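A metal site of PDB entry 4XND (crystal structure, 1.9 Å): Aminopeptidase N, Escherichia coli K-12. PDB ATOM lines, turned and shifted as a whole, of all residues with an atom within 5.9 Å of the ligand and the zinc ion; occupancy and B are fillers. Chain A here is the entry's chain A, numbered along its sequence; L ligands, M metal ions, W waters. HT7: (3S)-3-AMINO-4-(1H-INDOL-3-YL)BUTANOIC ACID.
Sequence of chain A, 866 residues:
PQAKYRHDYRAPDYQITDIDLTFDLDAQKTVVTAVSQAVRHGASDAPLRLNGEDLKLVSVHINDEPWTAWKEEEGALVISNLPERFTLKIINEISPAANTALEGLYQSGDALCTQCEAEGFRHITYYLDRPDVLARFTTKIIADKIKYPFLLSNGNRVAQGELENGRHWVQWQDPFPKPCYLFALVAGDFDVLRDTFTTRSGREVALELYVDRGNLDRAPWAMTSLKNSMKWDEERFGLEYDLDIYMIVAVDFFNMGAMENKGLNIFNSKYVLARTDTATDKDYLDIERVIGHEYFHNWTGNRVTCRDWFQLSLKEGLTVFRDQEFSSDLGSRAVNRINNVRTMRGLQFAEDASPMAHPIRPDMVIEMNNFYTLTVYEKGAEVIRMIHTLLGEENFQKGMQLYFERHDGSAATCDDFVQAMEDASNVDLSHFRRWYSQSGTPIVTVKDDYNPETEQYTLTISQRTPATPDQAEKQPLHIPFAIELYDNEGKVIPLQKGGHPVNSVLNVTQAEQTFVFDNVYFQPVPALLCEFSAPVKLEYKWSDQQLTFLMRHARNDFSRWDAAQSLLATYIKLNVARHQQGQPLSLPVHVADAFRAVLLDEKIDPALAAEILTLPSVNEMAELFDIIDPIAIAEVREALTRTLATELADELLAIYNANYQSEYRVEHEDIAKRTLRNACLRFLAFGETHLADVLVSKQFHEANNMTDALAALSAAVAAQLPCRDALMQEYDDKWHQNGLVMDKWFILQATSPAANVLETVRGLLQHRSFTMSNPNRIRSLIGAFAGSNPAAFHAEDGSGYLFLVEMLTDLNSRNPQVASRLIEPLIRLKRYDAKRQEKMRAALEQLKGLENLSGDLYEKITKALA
Water W1 bridges OE2 of Glu 103 and O of Glu 117.
Water W4 lies within hydrogen-bond range of O of Asn 369 (2.8 Å) and NE2 of Gln 817 (2.8 Å).
Residues that only touch the zinc ion: Tyr 377 (3.9 Å).
The zinc ion is bound by O of the ligand, 1.9 Å away.
The zinc ion is bound by OE1 of Glu 316, 1.9 Å away.
The zinc ion is bound by a ring nitrogen (NE2) of His 293, at 2.0 Å.
The zinc ion is bound by a ring nitrogen (NE2) of His 297 (2.1 Å).
The zinc ion has four donor atoms within binding distance.
Slightly farther from the zinc ion lies OXT of the ligand (2.7 Å).
Slightly farther from the zinc ion lies the side-chain carboxylate (OE2) of Glu 316 (2.8 Å).
The side-chain carboxylate (OE1) of Glu 260 is in salt-bridge range of a nitrogen (N) of the ligand.
The side-chain hydroxyl (OH) of Tyr 377 sits close to an oxygen (O) of the ligand (2.7 Å).
The side-chain carboxylate (OE1) of Glu 117 is in salt-bridge range of a nitrogen (N) of the ligand (2.8 Å).
The side-chain carboxylate of Glu 294 lies close to an oxygen (OXT) of the ligand (2.8 Å).
NE2 of Gln 115 sits close to NZ1 of the ligand (3.3 Å).
N of the ligand lies close to NZ of Lys 315, 3.5 Å away.
Merely in contact with the ligand: Ala 258 (3.1 Å), Asn 369 (3.3 Å), Met 256 (3.4 Å), Met 259 (3.6 Å) and Tyr 372 (3.7 Å).
Hydrophobic or aromatic side chains that line the ligand: Met 256, Met 259, His 293, His 297, Tyr 372 and Tyr 377.
14 residues have an atom within 4 Å of the ligand: Gln 115, Glu 117, Met 256, Ala 258, Met 259, Glu 260, His 293, Glu 294, His 297, Lys 315, Glu 316, Asn 369, Tyr 372 and Tyr 377.
The side-chain carboxylate of Glu 316 lies close to the side-chain hydroxyl of Tyr 377.
The side-chain hydroxyl of Thr 319 sits at hydrogen-bond distance from a ring nitrogen (ND1) of His 297.
OE2 of Glu 260 lies within salt-bridge range of NZ of Lys 315, at 2.9 Å.
The side-chain carboxylate (OE2) of Glu 117 is in salt-bridge range of the side-chain amino group (NZ) of Lys 315 (2.7 Å).
OE2 of Glu 117 sits at hydrogen-bond distance from OH of Tyr 372.
The side-chain amide nitrogen (ND2) of Asn 369 sits at hydrogen-bond distance from the side-chain carboxylate (OE2) of Glu 103 (3.1 Å).
The side-chain amide nitrogen (NE2) of Gln 817 lies within hydrogen-bond range of the side-chain sulfur (SD) of Met 256, at 3.3 Å.
The side-chain hydroxyl of Thr 319 sits at hydrogen-bond distance from the backbone carbonyl oxygen of Lys 315 (2.6 Å).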
ATOM      1  N   GLU A 103      -1.312  18.888  36.504  1.00  0.00           N
ATOM      2  CA  GLU A 103      -2.461  19.053  35.620  1.00  0.00           C
ATOM      3  C   GLU A 103      -2.330  20.472  35.058  1.00  0.00           C
ATOM      4  O   GLU A 103      -2.182  21.425  35.817  1.00  0.00           O
ATOM      5  CB  GLU A 103      -3.841  18.853  36.338  1.00  0.00           C
ATOM      6  CG  GLU A 103      -5.090  19.072  35.407  1.00  0.00           C
ATOM      7  CD  GLU A 103      -6.449  18.552  35.927  1.00  0.00           C
ATOM      8  OE1 GLU A 103      -6.978  19.247  36.777  1.00  0.00           O
ATOM      9  OE2 GLU A 103      -6.987  17.520  35.432  1.00  0.00           O
ATOM     10  N   GLN A 115      -0.329  18.351  30.926  1.00  0.00           N
ATOM     11  CA  GLN A 115      -1.300  17.275  30.831  1.00  0.00           C
ATOM     12  C   GLN A 115      -2.682  17.913  30.861  1.00  0.00           C
ATOM     13  O   GLN A 115      -3.011  18.602  31.873  1.00  0.00           O
ATOM     14  CB  GLN A 115      -1.115  16.318  32.031  1.00  0.00           C
ATOM     15  CG  GLN A 115      -2.221  15.248  32.129  1.00  0.00           C
ATOM     16  CD  GLN A 115      -2.363  14.424  30.883  1.00  0.00           C
ATOM     17  OE1 GLN A 115      -1.371  14.166  30.174  1.00  0.00           O
ATOM     18  NE2 GLN A 115      -3.586  14.016  30.579  1.00  0.00           N
ATOM     19  N   GLU A 117      -5.801  16.181  29.657  1.00  0.00           N
ATOM     20  CA  GLU A 117      -6.971  15.270  29.847  1.00  0.00           C
ATOM     21  C   GLU A 117      -7.110  15.064  31.356  1.00  0.00           C
ATOM     22  O   GLU A 117      -6.095  14.940  32.041  1.00  0.00           O
ATOM     23  CB  GLU A 117      -6.795  13.988  29.113  1.00  0.00           C
ATOM     24  CG  GLU A 117      -8.090  13.173  29.033  1.00  0.00           C
ATOM     25  CD  GLU A 117      -8.035  11.865  28.291  1.00  0.00           C
ATOM     26  OE1 GLU A 117      -7.048  11.607  27.568  1.00  0.00           O
ATOM     27  OE2 GLU A 117      -9.060  11.111  28.313  1.00  0.00           O
ATOM     28  N   ALA A 118      -8.331  15.131  31.897  1.00  0.00           N
ATOM     29  CA  ALA A 118      -9.583  15.387  31.149  1.00  0.00           C
ATOM     30  C   ALA A 118      -9.846  16.878  30.999  1.00  0.00           C
ATOM     31  O   ALA A 118     -10.237  17.338  29.897  1.00  0.00           O
ATOM     32  CB  ALA A 118     -10.774  14.775  31.891  1.00  0.00           C
ATOM     33  N   TYR A 181      -8.359  18.789  25.254  1.00  0.00           N
ATOM     34  CA  TYR A 181      -7.686  17.856  26.128  1.00  0.00           C
ATOM     35  C   TYR A 181      -6.507  17.235  25.353  1.00  0.00           C
ATOM     36  O   TYR A 181      -5.661  16.567  25.965  1.00  0.00           O
ATOM     37  CB  TYR A 181      -8.606  16.726  26.632  1.00  0.00           C
ATOM     38  CG  TYR A 181      -8.985  15.626  25.674  1.00  0.00           C
ATOM     39  CD1 TYR A 181      -8.165  14.470  25.537  1.00  0.00           C
ATOM     40  CD2 TYR A 181     -10.153  15.659  24.942  1.00  0.00           C
ATOM     41  CE1 TYR A 181      -8.603  13.399  24.756  1.00  0.00           C
ATOM     42  CE2 TYR A 181     -10.506  14.626  24.047  1.00  0.00           C
ATOM     43  CZ  TYR A 181      -9.707  13.494  23.958  1.00  0.00           C
ATOM     44  OH  TYR A 181     -10.040  12.464  23.131  1.00  0.00           O
ATOM     45  N   PHE A 254       4.731  12.413  36.024  1.00  0.00           N
ATOM     46  CA  PHE A 254       3.516  12.206  35.243  1.00  0.00           C
ATOM     47  C   PHE A 254       2.611  11.315  36.071  1.00  0.00           C
ATOM     48  O   PHE A 254       3.041  10.269  36.556  1.00  0.00           O
ATOM     49  CB  PHE A 254       3.913  11.471  33.933  1.00  0.00           C
ATOM     50  CG  PHE A 254       2.922  11.631  32.849  1.00  0.00           C
ATOM     51  CD1 PHE A 254       2.801  12.827  32.215  1.00  0.00           C
ATOM     52  CD2 PHE A 254       2.024  10.594  32.539  1.00  0.00           C
ATOM     53  CE1 PHE A 254       1.891  13.038  31.208  1.00  0.00           C
ATOM     54  CE2 PHE A 254       1.087  10.804  31.525  1.00  0.00           C
ATOM     55  CZ  PHE A 254       1.046  12.011  30.831  1.00  0.00           C
ATOM     56  N   ASN A 255       1.358  11.728  36.200  1.00  0.00           N
ATOM     57  CA  ASN A 255       0.406  10.986  37.018  1.00  0.00           C
ATOM     58  C   ASN A 255      -0.035   9.626  36.496  1.00  0.00           C
ATOM     59  O   ASN A 255      -0.234   8.713  37.297  1.00  0.00           O
ATOM     60  CB  ASN A 255      -0.807  11.852  37.313  1.00  0.00           C
ATOM     61  CG  ASN A 255      -0.526  12.923  38.315  1.00  0.00           C
ATOM     62  OD1 ASN A 255       0.390  12.785  39.140  1.00  0.00           O
ATOM     63  ND2 ASN A 255      -1.291  14.010  38.271  1.00  0.00           N
ATOM     64  N   MET A 256      -0.238   9.469  35.206  1.00  0.00           N
ATOM     65  CA  MET A 256      -0.649   8.163  34.703  1.00  0.00           C
ATOM     66  C   MET A 256       0.472   7.515  33.872  1.00  0.00           C
ATOM     67  O   MET A 256       1.623   7.803  34.129  1.00  0.00           O
ATOM     68  CB  MET A 256      -1.892   8.374  33.866  1.00  0.00           C
ATOM     69  CG  MET A 256      -3.028   8.924  34.713  1.00  0.00           C
ATOM     70  SD  MET A 256      -3.923   7.616  35.520  1.00  0.00           S
ATOM     71  CE  MET A 256      -5.059   7.374  34.158  1.00  0.00           C
ATOM     72  N   GLY A 257       0.141   6.749  32.854  1.00  0.00           N
ATOM     73  CA  GLY A 257       1.170   6.071  32.044  1.00  0.00           C
ATOM     74  C   GLY A 257       1.640   6.911  30.888  1.00  0.00           C
ATOM     75  O   GLY A 257       2.848   7.018  30.644  1.00  0.00           O
ATOM     76  N   ALA A 258       0.681   7.462  30.159  1.00  0.00           N
ATOM     77  CA  ALA A 258       1.042   8.264  28.977  1.00  0.00           C
ATOM     78  C   ALA A 258      -0.193   8.968  28.461  1.00  0.00           C
ATOM     79  O   ALA A 258      -1.258   8.808  29.019  1.00  0.00           O
ATOM     80  CB  ALA A 258       1.599   7.322  27.896  1.00  0.00           C
ATOM     81  N   MET A 259      -0.010   9.772  27.412  1.00  0.00           N
ATOM     82  CA  MET A 259      -1.104  10.591  26.930  1.00  0.00           C
ATOM     83  C   MET A 259      -1.026  10.806  25.401  1.00  0.00           C
ATOM     84  O   MET A 259       0.051  11.200  24.916  1.00  0.00           O
ATOM     85  CB  MET A 259      -1.111  11.928  27.678  1.00  0.00           C
ATOM     86  CG  MET A 259      -2.136  12.943  27.160  1.00  0.00           C
ATOM     87  SD  MET A 259      -3.819  12.354  27.439  1.00  0.00           S
ATOM     88  CE  MET A 259      -4.641  12.982  25.996  1.00  0.00           C
ATOM     89  N   GLU A 260      -2.157  10.563  24.701  1.00  0.00           N
ATOM     90  CA  GLU A 260      -2.195  10.530  23.262  1.00  0.00           C
ATOM     91  C   GLU A 260      -2.269  11.904  22.562  1.00  0.00           C
ATOM     92  O   GLU A 260      -2.898  12.027  21.522  1.00  0.00           O
ATOM     93  CB  GLU A 260      -3.341   9.651  22.817  1.00  0.00           C
ATOM     94  CG  GLU A 260      -4.736  10.244  23.170  1.00  0.00           C
ATOM     95  CD  GLU A 260      -5.354   9.732  24.500  1.00  0.00           C
ATOM     96  OE1 GLU A 260      -4.620   9.377  25.469  1.00  0.00           O
ATOM     97  OE2 GLU A 260      -6.648   9.803  24.599  1.00  0.00           O
ATOM     98  N   HIS A 293      -0.853   1.539  22.655  1.00  0.00           N
ATOM     99  CA  HIS A 293      -2.096   2.148  23.162  1.00  0.00           C
ATOM    100  C   HIS A 293      -2.158   3.602  22.727  1.00  0.00           C
ATOM    101  O   HIS A 293      -3.163   4.027  22.172  1.00  0.00           O
ATOM    102  CB  HIS A 293      -2.121   2.068  24.720  1.00  0.00           C
ATOM    103  CG  HIS A 293      -3.397   2.547  25.317  1.00  0.00           C
ATOM    104  ND1 HIS A 293      -4.461   1.716  25.598  1.00  0.00           N
ATOM    105  CD2 HIS A 293      -3.777   3.785  25.670  1.00  0.00           C
ATOM    106  CE1 HIS A 293      -5.460   2.460  26.043  1.00  0.00           C
ATOM    107  NE2 HIS A 293      -5.060   3.719  26.095  1.00  0.00           N
ATOM    108  N   GLU A 294      -1.132   4.379  22.990  1.00  0.00           N
ATOM    109  CA  GLU A 294      -1.197   5.854  22.629  1.00  0.00           C
ATOM    110  C   GLU A 294      -1.262   6.063  21.149  1.00  0.00           C
ATOM    111  O   GLU A 294      -2.005   6.917  20.660  1.00  0.00           O
ATOM    112  CB  GLU A 294      -0.021   6.632  23.232  1.00  0.00           C
ATOM    113  CG  GLU A 294       0.218   6.393  24.744  1.00  0.00           C
ATOM    114  CD  GLU A 294      -1.040   6.594  25.599  1.00  0.00           C
ATOM    115  OE1 GLU A 294      -1.907   7.428  25.228  1.00  0.00           O
ATOM    116  OE2 GLU A 294      -1.171   5.835  26.579  1.00  0.00           O
ATOM    117  N   HIS A 297      -4.791   5.368  19.801  1.00  0.00           N
ATOM    118  CA  HIS A 297      -5.671   6.490  20.098  1.00  0.00           C
ATOM    119  C   HIS A 297      -5.714   7.492  18.935  1.00  0.00           C
ATOM    120  O   HIS A 297      -6.645   8.308  18.855  1.00  0.00           O
ATOM    121  CB  HIS A 297      -5.256   7.244  21.334  1.00  0.00           C
ATOM    122  CG  HIS A 297      -5.884   6.770  22.614  1.00  0.00           C
ATOM    123  ND1 HIS A 297      -7.252   6.628  22.773  1.00  0.00           N
ATOM    124  CD2 HIS A 297      -5.331   6.549  23.828  1.00  0.00           C
ATOM    125  CE1 HIS A 297      -7.500   6.352  24.052  1.00  0.00           C
ATOM    126  NE2 HIS A 297      -6.362   6.246  24.678  1.00  0.00           N
ATOM    127  N   LYS A 315     -13.470   5.688  23.643  1.00  0.00           N
ATOM    128  CA  LYS A 315     -12.067   5.638  23.277  1.00  0.00           C
ATOM    129  C   LYS A 315     -11.242   4.644  24.132  1.00  0.00           C
ATOM    130  O   LYS A 315     -10.351   4.022  23.609  1.00  0.00           O
ATOM    131  CB  LYS A 315     -11.353   7.020  23.226  1.00  0.00           C
ATOM    132  CG  LYS A 315     -11.137   7.824  24.525  1.00  0.00           C
ATOM    133  CD  LYS A 315     -10.539   9.183  24.235  1.00  0.00           C
ATOM    134  CE  LYS A 315     -10.195   9.981  25.461  1.00  0.00           C
ATOM    135  NZ  LYS A 315      -8.998   9.515  26.191  1.00  0.00           N
ATOM    136  N   GLU A 316     -11.498   4.590  25.447  1.00  0.00           N
ATOM    137  CA  GLU A 316     -10.665   3.757  26.277  1.00  0.00           C
ATOM    138  C   GLU A 316     -10.919   2.251  26.164  1.00  0.00           C
ATOM    139  O   GLU A 316      -9.968   1.484  26.037  1.00  0.00           O
ATOM    140  CB  GLU A 316     -10.608   4.230  27.734  1.00  0.00           C
ATOM    141  CG  GLU A 316     -10.074   5.694  27.930  1.00  0.00           C
ATOM    142  CD  GLU A 316      -8.702   5.893  27.332  1.00  0.00           C
ATOM    143  OE1 GLU A 316      -8.011   4.900  27.017  1.00  0.00           O
ATOM    144  OE2 GLU A 316      -8.345   7.059  27.129  1.00  0.00           O
ATOM    145  N   THR A 319      -9.631   1.372  22.644  1.00  0.00           N
ATOM    146  CA  THR A 319      -8.156   1.445  22.560  1.00  0.00           C
ATOM    147  C   THR A 319      -7.463   0.413  23.396  1.00  0.00           C
ATOM    148  O   THR A 319      -6.467  -0.158  22.944  1.00  0.00           O
ATOM    149  CB  THR A 319      -7.641   2.882  22.807  1.00  0.00           C
ATOM    150  OG1 THR A 319      -8.347   3.790  21.921  1.00  0.00           O
ATOM    151  CG2 THR A 319      -6.135   2.987  22.654  1.00  0.00           C
ATOM    152  N   VAL A 320      -8.024   0.075  24.562  1.00  0.00           N
ATOM    153  CA  VAL A 320      -7.493  -1.104  25.275  1.00  0.00           C
ATOM    154  C   VAL A 320      -7.686  -2.384  24.471  1.00  0.00           C
ATOM    155  O   VAL A 320      -6.751  -3.217  24.418  1.00  0.00           O
ATOM    156  CB  VAL A 320      -8.112  -1.203  26.675  1.00  0.00           C
ATOM    157  CG1 VAL A 320      -7.684  -2.547  27.352  1.00  0.00           C
ATOM    158  CG2 VAL A 320      -7.658  -0.031  27.526  1.00  0.00           C
ATOM    159  N   ASN A 369     -11.458  12.853  36.830  1.00  0.00           N
ATOM    160  CA  ASN A 369     -10.234  12.087  36.984  1.00  0.00           C
ATOM    161  C   ASN A 369     -10.379  10.781  37.766  1.00  0.00           C
ATOM    162  O   ASN A 369      -9.578   9.842  37.587  1.00  0.00           O
ATOM    163  CB  ASN A 369      -9.123  12.947  37.543  1.00  0.00           C
ATOM    164  CG  ASN A 369      -8.665  14.028  36.497  1.00  0.00           C
ATOM    165  OD1 ASN A 369      -9.013  14.008  35.338  1.00  0.00           O
ATOM    166  ND2 ASN A 369      -7.885  14.948  36.972  1.00  0.00           N
ATOM    167  N   TYR A 372     -11.032   7.243  35.295  1.00  0.00           N
ATOM    168  CA  TYR A 372     -10.028   6.535  34.471  1.00  0.00           C
ATOM    169  C   TYR A 372      -9.786   5.164  35.137  1.00  0.00           C
ATOM    170  O   TYR A 372      -8.769   4.981  35.795  1.00  0.00           O
ATOM    171  CB  TYR A 372      -8.787   7.417  34.350  1.00  0.00           C
ATOM    172  CG  TYR A 372      -9.144   8.559  33.382  1.00  0.00           C
ATOM    173  CD1 TYR A 372      -9.902   9.683  33.805  1.00  0.00           C
ATOM    174  CD2 TYR A 372      -8.828   8.475  32.049  1.00  0.00           C
ATOM    175  CE1 TYR A 372     -10.264  10.672  32.905  1.00  0.00           C
ATOM    176  CE2 TYR A 372      -9.188   9.460  31.170  1.00  0.00           C
ATOM    177  CZ  TYR A 372      -9.957  10.561  31.613  1.00  0.00           C
ATOM    178  OH  TYR A 372     -10.351  11.532  30.693  1.00  0.00           O
ATOM    179  N   TYR A 377     -11.791   1.115  31.356  1.00  0.00           N
ATOM    180  CA  TYR A 377     -10.717   0.552  30.498  1.00  0.00           C
ATOM    181  C   TYR A 377     -10.854  -0.947  30.233  1.00  0.00           C
ATOM    182  O   TYR A 377     -11.081  -1.382  29.082  1.00  0.00           O
ATOM    183  CB  TYR A 377      -9.333   0.836  31.086  1.00  0.00           C
ATOM    184  CG  TYR A 377      -8.781   2.238  30.889  1.00  0.00           C
ATOM    185  CD1 TYR A 377      -9.408   3.353  31.459  1.00  0.00           C
ATOM    186  CD2 TYR A 377      -7.639   2.454  30.129  1.00  0.00           C
ATOM    187  CE1 TYR A 377      -8.870   4.622  31.280  1.00  0.00           C
ATOM    188  CE2 TYR A 377      -7.078   3.706  29.944  1.00  0.00           C
ATOM    189  CZ  TYR A 377      -7.728   4.814  30.491  1.00  0.00           C
ATOM    190  OH  TYR A 377      -7.228   6.093  30.286  1.00  0.00           O
ATOM    191  N   GLN A 817      -4.914  13.703  42.369  1.00  0.00           N
ATOM    192  CA  GLN A 817      -5.084  12.543  41.515  1.00  0.00           C
ATOM    193  C   GLN A 817      -4.366  11.315  42.067  1.00  0.00           C
ATOM    194  O   GLN A 817      -4.887  10.200  42.071  1.00  0.00           O
ATOM    195  CB  GLN A 817      -4.525  12.889  40.122  1.00  0.00           C
ATOM    196  CG  GLN A 817      -4.929  11.967  39.008  1.00  0.00           C
ATOM    197  CD  GLN A 817      -4.052  10.701  38.859  1.00  0.00           C
ATOM    198  OE1 GLN A 817      -3.005  10.520  39.537  1.00  0.00           O
ATOM    199  NE2 GLN A 817      -4.479   9.823  37.978  1.00  0.00           N
HETATM  200  N   HT7 L   1      -5.887   9.115  27.690  1.00  0.00           N
HETATM  201  CB  HT7 L   1      -4.875   9.240  28.799  1.00  0.00           C
HETATM  202  CG  HT7 L   1      -5.564   9.850  30.045  1.00  0.00           C
HETATM  203  CD  HT7 L   1      -4.692  10.502  31.096  1.00  0.00           C
HETATM  204  CE2 HT7 L   1      -5.159  11.136  32.261  1.00  0.00           C
HETATM  205  CZ3 HT7 L   1      -6.459  11.431  32.741  1.00  0.00           C
HETATM  206  CH3 HT7 L   1      -6.607  12.138  33.966  1.00  0.00           C
HETATM  207  CT2 HT7 L   1      -5.479  12.561  34.688  1.00  0.00           C
HETATM  208  CH2 HT7 L   1      -4.196  12.306  34.182  1.00  0.00           C
HETATM  209  CZ2 HT7 L   1      -4.045  11.604  32.949  1.00  0.00           C
HETATM  210  NZ1 HT7 L   1      -2.923  11.255  32.221  1.00  0.00           N
HETATM  211  CE1 HT7 L   1      -3.293  10.571  31.115  1.00  0.00           C
HETATM  212  CA  HT7 L   1      -4.207   7.894  29.186  1.00  0.00           C
HETATM  213  C   HT7 L   1      -4.537   6.878  28.136  1.00  0.00           C
HETATM  214  O   HT7 L   1      -5.634   6.139  28.128  1.00  0.00           O
HETATM  215  OXT HT7 L   1      -3.926   6.754  27.089  1.00  0.00           O
HETATM  216 ZN    ZN M   1      -6.191   5.338  26.522  1.00  0.00          ZN
HETATM  217  O   HOH W   1      -5.107  15.857  34.423  1.00  0.00           O
HETATM  218  O   HOH W   2      -2.703  15.028  35.683  1.00  0.00           O
HETATM  219  O   HOH W   3      -0.682  12.450  33.712  1.00  0.00           O
HETATM  220  O   HOH W   4      -6.947   9.992  36.591  1.00  0.00           O
